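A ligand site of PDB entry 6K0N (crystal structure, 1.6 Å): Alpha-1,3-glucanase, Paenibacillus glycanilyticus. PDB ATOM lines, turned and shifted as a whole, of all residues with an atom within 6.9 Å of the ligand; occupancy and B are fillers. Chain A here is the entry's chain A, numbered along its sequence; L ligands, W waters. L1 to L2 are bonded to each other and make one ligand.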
ATOM      1  N   TYR A 122     -23.865 -21.127  18.966  1.00  0.00           N
ATOM      2  CA  TYR A 122     -23.497 -21.380  20.358  1.00  0.00           C
ATOM      3  C   TYR A 122     -24.622 -21.929  21.222  1.00  0.00           C
ATOM      4  O   TYR A 122     -24.350 -22.598  22.226  1.00  0.00           O
ATOM      5  CB  TYR A 122     -22.988 -20.095  21.013  1.00  0.00           C
ATOM      6  CG  TYR A 122     -21.590 -19.673  20.631  1.00  0.00           C
ATOM      7  CD1 TYR A 122     -20.483 -20.192  21.280  1.00  0.00           C
ATOM      8  CD2 TYR A 122     -21.379 -18.733  19.628  1.00  0.00           C
ATOM      9  CE1 TYR A 122     -19.191 -19.805  20.930  1.00  0.00           C
ATOM     10  CE2 TYR A 122     -20.106 -18.335  19.272  1.00  0.00           C
ATOM     11  CZ  TYR A 122     -19.014 -18.867  19.930  1.00  0.00           C
ATOM     12  OH  TYR A 122     -17.746 -18.473  19.582  1.00  0.00           O
ATOM     13  N   ARG A 280     -21.569 -24.987  19.318  1.00  0.00           N
ATOM     14  CA  ARG A 280     -20.164 -24.580  19.326  1.00  0.00           C
ATOM     15  C   ARG A 280     -19.648 -24.447  20.754  1.00  0.00           C
ATOM     16  O   ARG A 280     -20.348 -23.938  21.645  1.00  0.00           O
ATOM     17  CB  ARG A 280     -20.022 -23.248  18.592  1.00  0.00           C
ATOM     18  CG  ARG A 280     -18.633 -22.695  18.528  1.00  0.00           C
ATOM     19  CD  ARG A 280     -18.616 -21.479  17.623  1.00  0.00           C
ATOM     20  NE  ARG A 280     -17.293 -20.853  17.585  1.00  0.00           N
ATOM     21  CZ  ARG A 280     -16.897 -20.010  16.631  1.00  0.00           C
ATOM     22  NH1 ARG A 280     -17.709 -19.674  15.647  1.00  0.00           N
ATOM     23  NH2 ARG A 280     -15.669 -19.503  16.675  1.00  0.00           N
ATOM     24  N   VAL A 281     -18.432 -24.932  20.967  1.00  0.00           N
ATOM     25  CA  VAL A 281     -17.677 -24.713  22.202  1.00  0.00           C
ATOM     26  C   VAL A 281     -16.282 -24.291  21.792  1.00  0.00           C
ATOM     27  O   VAL A 281     -15.672 -24.924  20.919  1.00  0.00           O
ATOM     28  CB  VAL A 281     -17.635 -25.970  23.096  1.00  0.00           C
ATOM     29  CG1 VAL A 281     -16.968 -25.661  24.443  1.00  0.00           C
ATOM     30  CG2 VAL A 281     -19.039 -26.518  23.310  1.00  0.00           C
ATOM     31  N   ASP A 282     -15.777 -23.212  22.394  1.00  0.00           N
ATOM     32  CA  ASP A 282     -14.487 -22.671  21.998  1.00  0.00           C
ATOM     33  C   ASP A 282     -13.395 -23.216  22.912  1.00  0.00           C
ATOM     34  O   ASP A 282     -13.406 -22.955  24.115  1.00  0.00           O
ATOM     35  CB  ASP A 282     -14.504 -21.146  22.006  1.00  0.00           C
ATOM     36  CG  ASP A 282     -15.377 -20.557  20.915  1.00  0.00           C
ATOM     37  OD1 ASP A 282     -15.587 -21.222  19.882  1.00  0.00           O
ATOM     38  OD2 ASP A 282     -15.855 -19.422  21.093  1.00  0.00           O
ATOM     39  N   GLY A 283     -12.477 -23.976  22.333  1.00  0.00           N
ATOM     40  CA  GLY A 283     -11.444 -24.662  23.078  1.00  0.00           C
ATOM     41  C   GLY A 283     -11.364 -26.115  22.651  1.00  0.00           C
ATOM     42  O   GLY A 283     -10.573 -26.487  21.778  1.00  0.00           O
ATOM     43  N   PRO A 284     -12.212 -26.954  23.240  1.00  0.00           N
ATOM     44  CA  PRO A 284     -12.332 -28.334  22.780  1.00  0.00           C
ATOM     45  C   PRO A 284     -13.081 -28.403  21.450  1.00  0.00           C
ATOM     46  O   PRO A 284     -13.611 -27.404  20.953  1.00  0.00           O
ATOM     47  CB  PRO A 284     -13.136 -29.012  23.895  1.00  0.00           C
ATOM     48  CG  PRO A 284     -14.004 -27.901  24.427  1.00  0.00           C
ATOM     49  CD  PRO A 284     -13.121 -26.664  24.360  1.00  0.00           C
ATOM     50  N   LYS A 286     -12.071 -30.069  18.267  1.00  0.00           N
ATOM     51  CA  LYS A 286     -11.450 -30.350  16.981  1.00  0.00           C
ATOM     52  C   LYS A 286     -11.269 -31.854  16.866  1.00  0.00           C
ATOM     53  O   LYS A 286     -10.779 -32.498  17.800  1.00  0.00           O
ATOM     54  CB  LYS A 286     -10.106 -29.625  16.854  1.00  0.00           C
ATOM     55  CG  LYS A 286     -10.232 -28.117  16.744  1.00  0.00           C
ATOM     56  CD  LYS A 286     -10.120 -27.445  18.113  1.00  0.00           C
ATOM     57  CE  LYS A 286     -10.100 -25.932  17.954  1.00  0.00           C
ATOM     58  NZ  LYS A 286      -9.860 -25.245  19.269  1.00  0.00           N
ATOM     59  N   ASN A 291      -1.006 -29.763  17.718  1.00  0.00           N
ATOM     60  CA  ASN A 291      -0.323 -28.476  17.788  1.00  0.00           C
ATOM     61  C   ASN A 291       1.144 -28.639  17.398  1.00  0.00           C
ATOM     62  O   ASN A 291       1.850 -29.500  17.940  1.00  0.00           O
ATOM     63  CB  ASN A 291      -0.491 -27.862  19.169  1.00  0.00           C
ATOM     64  CG  ASN A 291      -1.871 -27.247  19.359  1.00  0.00           C
ATOM     65  OD1 ASN A 291      -2.757 -27.400  18.511  1.00  0.00           O
ATOM     66  ND2 ASN A 291      -2.064 -26.536  20.463  1.00  0.00           N
ATOM     67  N   VAL A 307     -16.553 -29.275  16.331  1.00  0.00           N
ATOM     68  CA  VAL A 307     -16.382 -27.835  16.174  1.00  0.00           C
ATOM     69  C   VAL A 307     -15.537 -27.541  14.936  1.00  0.00           C
ATOM     70  O   VAL A 307     -15.924 -26.730  14.096  1.00  0.00           O
ATOM     71  CB  VAL A 307     -15.769 -27.231  17.457  1.00  0.00           C
ATOM     72  CG1 VAL A 307     -15.614 -25.726  17.301  1.00  0.00           C
ATOM     73  CG2 VAL A 307     -16.694 -27.534  18.639  1.00  0.00           C
ATOM     74  N   CYS A 308     -14.422 -28.255  14.772  1.00  0.00           N
ATOM     75  CA  CYS A 308     -13.579 -28.132  13.579  1.00  0.00           C
ATOM     76  C   CYS A 308     -13.061 -29.504  13.175  1.00  0.00           C
ATOM     77  O   CYS A 308     -13.012 -30.431  13.984  1.00  0.00           O
ATOM     78  CB  CYS A 308     -12.348 -27.234  13.807  1.00  0.00           C
ATOM     79  SG  CYS A 308     -12.652 -25.643  14.535  1.00  0.00           S
ATOM     80  N   TRP A 311      -7.360 -27.419  13.598  1.00  0.00           N
ATOM     81  CA  TRP A 311      -6.996 -26.042  13.937  1.00  0.00           C
ATOM     82  C   TRP A 311      -5.493 -26.043  14.171  1.00  0.00           C
ATOM     83  O   TRP A 311      -5.038 -26.326  15.286  1.00  0.00           O
ATOM     84  CB  TRP A 311      -7.770 -25.558  15.147  1.00  0.00           C
ATOM     85  CG  TRP A 311      -7.524 -24.123  15.495  1.00  0.00           C
ATOM     86  CD1 TRP A 311      -6.410 -23.582  16.102  1.00  0.00           C
ATOM     87  CD2 TRP A 311      -8.434 -23.033  15.293  1.00  0.00           C
ATOM     88  NE1 TRP A 311      -6.577 -22.224  16.276  1.00  0.00           N
ATOM     89  CE2 TRP A 311      -7.806 -21.862  15.775  1.00  0.00           C
ATOM     90  CE3 TRP A 311      -9.711 -22.936  14.731  1.00  0.00           C
ATOM     91  CZ2 TRP A 311      -8.421 -20.608  15.735  1.00  0.00           C
ATOM     92  CZ3 TRP A 311     -10.321 -21.691  14.676  1.00  0.00           C
ATOM     93  CH2 TRP A 311      -9.677 -20.547  15.179  1.00  0.00           C
ATOM     94  N   VAL A 313      -1.615 -24.965  14.755  1.00  0.00           N
ATOM     95  CA  VAL A 313      -0.868 -23.984  15.522  1.00  0.00           C
ATOM     96  C   VAL A 313       0.610 -24.234  15.259  1.00  0.00           C
ATOM     97  O   VAL A 313       1.181 -25.202  15.773  1.00  0.00           O
ATOM     98  CB  VAL A 313      -1.163 -24.055  17.026  1.00  0.00           C
ATOM     99  CG1 VAL A 313      -0.443 -22.925  17.728  1.00  0.00           C
ATOM    100  CG2 VAL A 313      -2.660 -23.986  17.280  1.00  0.00           C
ATOM    101  N   PHE A 329     -19.478 -26.870  13.813  1.00  0.00           N
ATOM    102  CA  PHE A 329     -19.983 -25.750  14.582  1.00  0.00           C
ATOM    103  C   PHE A 329     -19.040 -24.545  14.588  1.00  0.00           C
ATOM    104  O   PHE A 329     -19.454 -23.465  15.038  1.00  0.00           O
ATOM    105  CB  PHE A 329     -20.348 -26.220  16.001  1.00  0.00           C
ATOM    106  CG  PHE A 329     -21.568 -27.094  15.978  1.00  0.00           C
ATOM    107  CD1 PHE A 329     -22.824 -26.526  16.023  1.00  0.00           C
ATOM    108  CD2 PHE A 329     -21.451 -28.452  15.774  1.00  0.00           C
ATOM    109  CE1 PHE A 329     -23.963 -27.319  15.927  1.00  0.00           C
ATOM    110  CE2 PHE A 329     -22.578 -29.260  15.677  1.00  0.00           C
ATOM    111  CZ  PHE A 329     -23.844 -28.676  15.751  1.00  0.00           C
ATOM    112  N   ALA A 330     -17.830 -24.690  14.057  1.00  0.00           N
ATOM    113  CA  ALA A 330     -16.988 -23.549  13.739  1.00  0.00           C
ATOM    114  C   ALA A 330     -16.210 -23.845  12.454  1.00  0.00           C
ATOM    115  O   ALA A 330     -16.756 -24.493  11.557  1.00  0.00           O
ATOM    116  CB  ALA A 330     -16.050 -23.204  14.899  1.00  0.00           C
ATOM    117  N   ASP A 331     -14.955 -23.399  12.376  1.00  0.00           N
ATOM    118  CA  ASP A 331     -14.172 -23.502  11.136  1.00  0.00           C
ATOM    119  C   ASP A 331     -14.050 -24.945  10.677  1.00  0.00           C
ATOM    120  O   ASP A 331     -14.024 -25.877  11.481  1.00  0.00           O
ATOM    121  CB  ASP A 331     -12.735 -22.963  11.331  1.00  0.00           C
ATOM    122  CG  ASP A 331     -12.677 -21.545  11.852  1.00  0.00           C
ATOM    123  OD1 ASP A 331     -13.433 -21.200  12.773  1.00  0.00           O
ATOM    124  OD2 ASP A 331     -11.804 -20.782  11.355  1.00  0.00           O
ATOM    125  N   ASN A 334      -8.489 -24.497   9.851  1.00  0.00           N
ATOM    126  CA  ASN A 334      -7.786 -23.239  10.063  1.00  0.00           C
ATOM    127  C   ASN A 334      -6.337 -23.582  10.373  1.00  0.00           C
ATOM    128  O   ASN A 334      -6.070 -24.583  11.042  1.00  0.00           O
ATOM    129  CB  ASN A 334      -8.418 -22.433  11.204  1.00  0.00           C
ATOM    130  CG  ASN A 334      -8.020 -20.960  11.211  1.00  0.00           C
ATOM    131  OD1 ASN A 334      -7.170 -20.520  10.438  1.00  0.00           O
ATOM    132  ND2 ASN A 334      -8.662 -20.186  12.078  1.00  0.00           N
ATOM    133  N   THR A 336      -2.937 -21.651  11.842  1.00  0.00           N
ATOM    134  CA  THR A 336      -2.639 -20.396  12.515  1.00  0.00           C
ATOM    135  C   THR A 336      -1.187 -20.360  12.988  1.00  0.00           C
ATOM    136  O   THR A 336      -0.469 -21.363  12.986  1.00  0.00           O
ATOM    137  CB  THR A 336      -3.550 -20.151  13.714  1.00  0.00           C
ATOM    138  OG1 THR A 336      -3.060 -20.907  14.835  1.00  0.00           O
ATOM    139  CG2 THR A 336      -4.986 -20.556  13.424  1.00  0.00           C
ATOM    140  N   ASN A 337      -0.773 -19.151  13.382  1.00  0.00           N
ATOM    141  CA  ASN A 337       0.363 -18.929  14.271  1.00  0.00           C
ATOM    142  C   ASN A 337       1.629 -19.633  13.787  1.00  0.00           C
ATOM    143  O   ASN A 337       2.253 -20.402  14.513  1.00  0.00           O
ATOM    144  CB  ASN A 337       0.007 -19.353  15.695  1.00  0.00           C
ATOM    145  CG  ASN A 337      -1.145 -18.562  16.273  1.00  0.00           C
ATOM    146  OD1 ASN A 337      -1.814 -17.804  15.552  1.00  0.00           O
ATOM    147  ND2 ASN A 337      -1.384 -18.719  17.569  1.00  0.00           N
ATOM    148  N   ASP A 354     -18.229 -21.577  11.001  1.00  0.00           N
ATOM    149  CA  ASP A 354     -17.381 -20.392  10.909  1.00  0.00           C
ATOM    150  C   ASP A 354     -16.605 -20.574   9.608  1.00  0.00           C
ATOM    151  O   ASP A 354     -16.943 -21.457   8.803  1.00  0.00           O
ATOM    152  CB  ASP A 354     -16.511 -20.223  12.163  1.00  0.00           C
ATOM    153  CG  ASP A 354     -16.173 -18.749  12.460  1.00  0.00           C
ATOM    154  OD1 ASP A 354     -15.586 -18.066  11.592  1.00  0.00           O
ATOM    155  OD2 ASP A 354     -16.491 -18.267  13.579  1.00  0.00           O
ATOM    156  N   PHE A 360      -4.795 -18.025   9.432  1.00  0.00           N
ATOM    157  CA  PHE A 360      -4.622 -16.881  10.318  1.00  0.00           C
ATOM    158  C   PHE A 360      -3.149 -16.743  10.652  1.00  0.00           C
ATOM    159  O   PHE A 360      -2.605 -17.554  11.421  1.00  0.00           O
ATOM    160  CB  PHE A 360      -5.445 -17.005  11.601  1.00  0.00           C
ATOM    161  CG  PHE A 360      -5.423 -15.749  12.441  1.00  0.00           C
ATOM    162  CD1 PHE A 360      -4.382 -15.500  13.323  1.00  0.00           C
ATOM    163  CD2 PHE A 360      -6.432 -14.807  12.329  1.00  0.00           C
ATOM    164  CE1 PHE A 360      -4.351 -14.334  14.079  1.00  0.00           C
ATOM    165  CE2 PHE A 360      -6.406 -13.646  13.078  1.00  0.00           C
ATOM    166  CZ  PHE A 360      -5.383 -13.410  13.955  1.00  0.00           C
ATOM    167  N   TYR A 422      -4.407 -10.190  18.570  1.00  0.00           N
ATOM    168  CA  TYR A 422      -3.271 -11.091  18.642  1.00  0.00           C
ATOM    169  C   TYR A 422      -2.020 -10.406  18.105  1.00  0.00           C
ATOM    170  O   TYR A 422      -2.059  -9.270  17.604  1.00  0.00           O
ATOM    171  CB  TYR A 422      -3.569 -12.380  17.870  1.00  0.00           C
ATOM    172  CG  TYR A 422      -4.787 -13.128  18.405  1.00  0.00           C
ATOM    173  CD1 TYR A 422      -4.723 -13.820  19.605  1.00  0.00           C
ATOM    174  CD2 TYR A 422      -5.981 -13.164  17.703  1.00  0.00           C
ATOM    175  CE1 TYR A 422      -5.815 -14.503  20.100  1.00  0.00           C
ATOM    176  CE2 TYR A 422      -7.092 -13.848  18.185  1.00  0.00           C
ATOM    177  CZ  TYR A 422      -7.000 -14.518  19.389  1.00  0.00           C
ATOM    178  OH  TYR A 422      -8.086 -15.209  19.883  1.00  0.00           O
HETATM  179  C1  LIG L   1     -12.491 -19.054  18.534  1.00  0.00           C
HETATM  180  C2  LIG L   1     -11.330 -19.366  19.465  1.00  0.00           C
HETATM  181  C3  LIG L   1     -10.466 -20.477  18.891  1.00  0.00           C
HETATM  182  C4  LIG L   1     -11.313 -21.704  18.578  1.00  0.00           C
HETATM  183  C5  LIG L   1     -12.452 -21.285  17.643  1.00  0.00           C
HETATM  184  C6  LIG L   1     -13.371 -22.468  17.336  1.00  0.00           C
HETATM  185  O1  LIG L   1     -12.008 -18.513  17.308  1.00  0.00           O
HETATM  186  O2  LIG L   1     -10.552 -18.173  19.635  1.00  0.00           O
HETATM  187  O3  LIG L   1      -9.442 -20.821  19.835  1.00  0.00           O
HETATM  188  O4  LIG L   1     -10.529 -22.723  17.953  1.00  0.00           O
HETATM  189  O5  LIG L   1     -13.219 -20.253  18.274  1.00  0.00           O
HETATM  190  O6  LIG L   1     -13.951 -22.983  18.541  1.00  0.00           O
HETATM  191  C1  LG2 L   2      -8.229 -21.247  19.344  1.00  0.00           C
HETATM  192  C2  LG2 L   2      -7.365 -21.907  20.416  1.00  0.00           C
HETATM  193  C3  LG2 L   2      -6.947 -20.856  21.445  1.00  0.00           C
HETATM  194  C4  LG2 L   2      -6.258 -19.689  20.743  1.00  0.00           C
HETATM  195  C5  LG2 L   2      -7.169 -19.143  19.642  1.00  0.00           C
HETATM  196  C6  LG2 L   2      -6.543 -17.973  18.889  1.00  0.00           C
HETATM  197  O1  LG2 L   2      -8.103 -22.955  21.049  1.00  0.00           O
HETATM  198  O2  LG2 L   2      -6.073 -21.451  22.415  1.00  0.00           O
HETATM  199  O3  LG2 L   2      -5.979 -18.656  21.699  1.00  0.00           O
HETATM  200  O4  LG2 L   2      -7.485 -20.194  18.718  1.00  0.00           O
HETATM  201  O5  LG2 L   2      -5.337 -18.369  18.214  1.00  0.00           O
HETATM  202  O   HOH W   1      -4.421 -20.574  17.279  1.00  0.00           O
HETATM  203  O   HOH W   2      -5.557 -17.485  15.618  1.00  0.00           O
HETATM  204  O   HOH W   3      -6.565 -24.798  22.225  1.00  0.00           O
HETATM  205  O   HOH W   4      -3.197 -17.366  21.035  1.00  0.00           O
HETATM  206  O   HOH W   5      -9.695 -16.752  17.621  1.00  0.00           O
HETATM  207  O   HOH W   6     -12.836 -25.052  19.766  1.00  0.00           O
HETATM  208  O   HOH W   7      -7.589 -22.098  24.799  1.00  0.00           O
HETATM  209  O   HOH W   8      -9.892 -21.779  23.118  1.00  0.00           O
HETATM  210  O   HOH W   9     -13.490 -19.137  14.634  1.00  0.00           O
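An oxygen (O6) of LIG L1 is in hydrogen-bond range of the side-chain carboxylate (OD1) of Asp 282 (2.8 Å). An oxygen (O5) of LIG L1 is in hydrogen-bond range of the guanidinium group (NH2) of Arg 280 (3.0 Å). NE1 of Trp 311 lies close to O4 of LG2 L2 (3.3 Å). An oxygen (O4) of LIG L1 sits at hydrogen-bond distance from the side-chain amino group of Lys 286, 2.9 Å away.
The guanidinium group of Arg 280 lies within salt-bridge range of the side-chain carboxylate of Asp 354 (2.8 Å). N of Asp 354 lies within hydrogen-bond range of O of Ala 330, at 3.3 Å. The side-chain hydroxyl (OH) of Tyr 122 is in hydrogen-bond range of the side-chain carboxylate (OD2) of Asp 282 (2.6 Å). OD1 of Asp 282 lies within salt-bridge range of NE of Arg 280 (2.9 Å). The side-chain amino group of Lys 286 is in hydrogen-bond range of the backbone carbonyl oxygen of Gly 283 (2.9 Å). The guanidinium group (NE) of Arg 280 is in hydrogen-bond range of the side-chain hydroxyl (OH) of Tyr 122 (3.1 Å). O of Val 307 is in hydrogen-bond range of N of Ala 330, 2.8 Å away.
O of Val 281 touches O6 of LIG L1, 3.5 Å away. CG1 of Val 307 touches O6 of LIG L1, 3.4 Å away. Ala 330 touches the ligand. OH of Tyr 422 touches C6 of LG2 L2, 3.3 Å away. Hydrophobic or aromatic side chains that line the ligand: Val 307, Trp 311, Ala 330 and Tyr 422. Of the 21 residues printed, 8 come within 4 Å of the ligand. The nearest printed residue that does not touch the ligand is Asn 337 (4.02 Å).
Water W1 lies within hydrogen-bond range of an oxygen (O5) of LG2 L2 (2.6 Å), the side-chain hydroxyl (OG1) of Thr 336 (2.8 Å) and the indole nitrogen (NE1) of Trp 311 (2.9 Å). Water W5 lies within hydrogen-bond range of an oxygen (O2) of LIG L1 and the side-chain hydroxyl (OH) of Tyr 422. Water W6 lies within hydrogen-bond range of an oxygen (O6) of LIG L1 (2.7 Å), the backbone carbonyl oxygen (O) of Pro 284 (2.7 Å), the backbone NH (N) of Gly 283 (2.8 Å), the side-chain amino group (NZ) of Lys 286 (3.0 Å) and the backbone carbonyl oxygen (O) of Val 281 (3.1 Å). Water W8 lies within hydrogen-bond range of an oxygen (O1) of LG2 L2 (3.0 Å) and the backbone NH of Gly 283 (3.5 Å). Water W9 lies within hydrogen-bond range of OD1 of Asp 331 (2.8 Å), NH2 of Arg 280 (3.0 Å), O1 of LIG L1 (3.1 Å) and OD2 of Asp 354 (3.3 Å).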
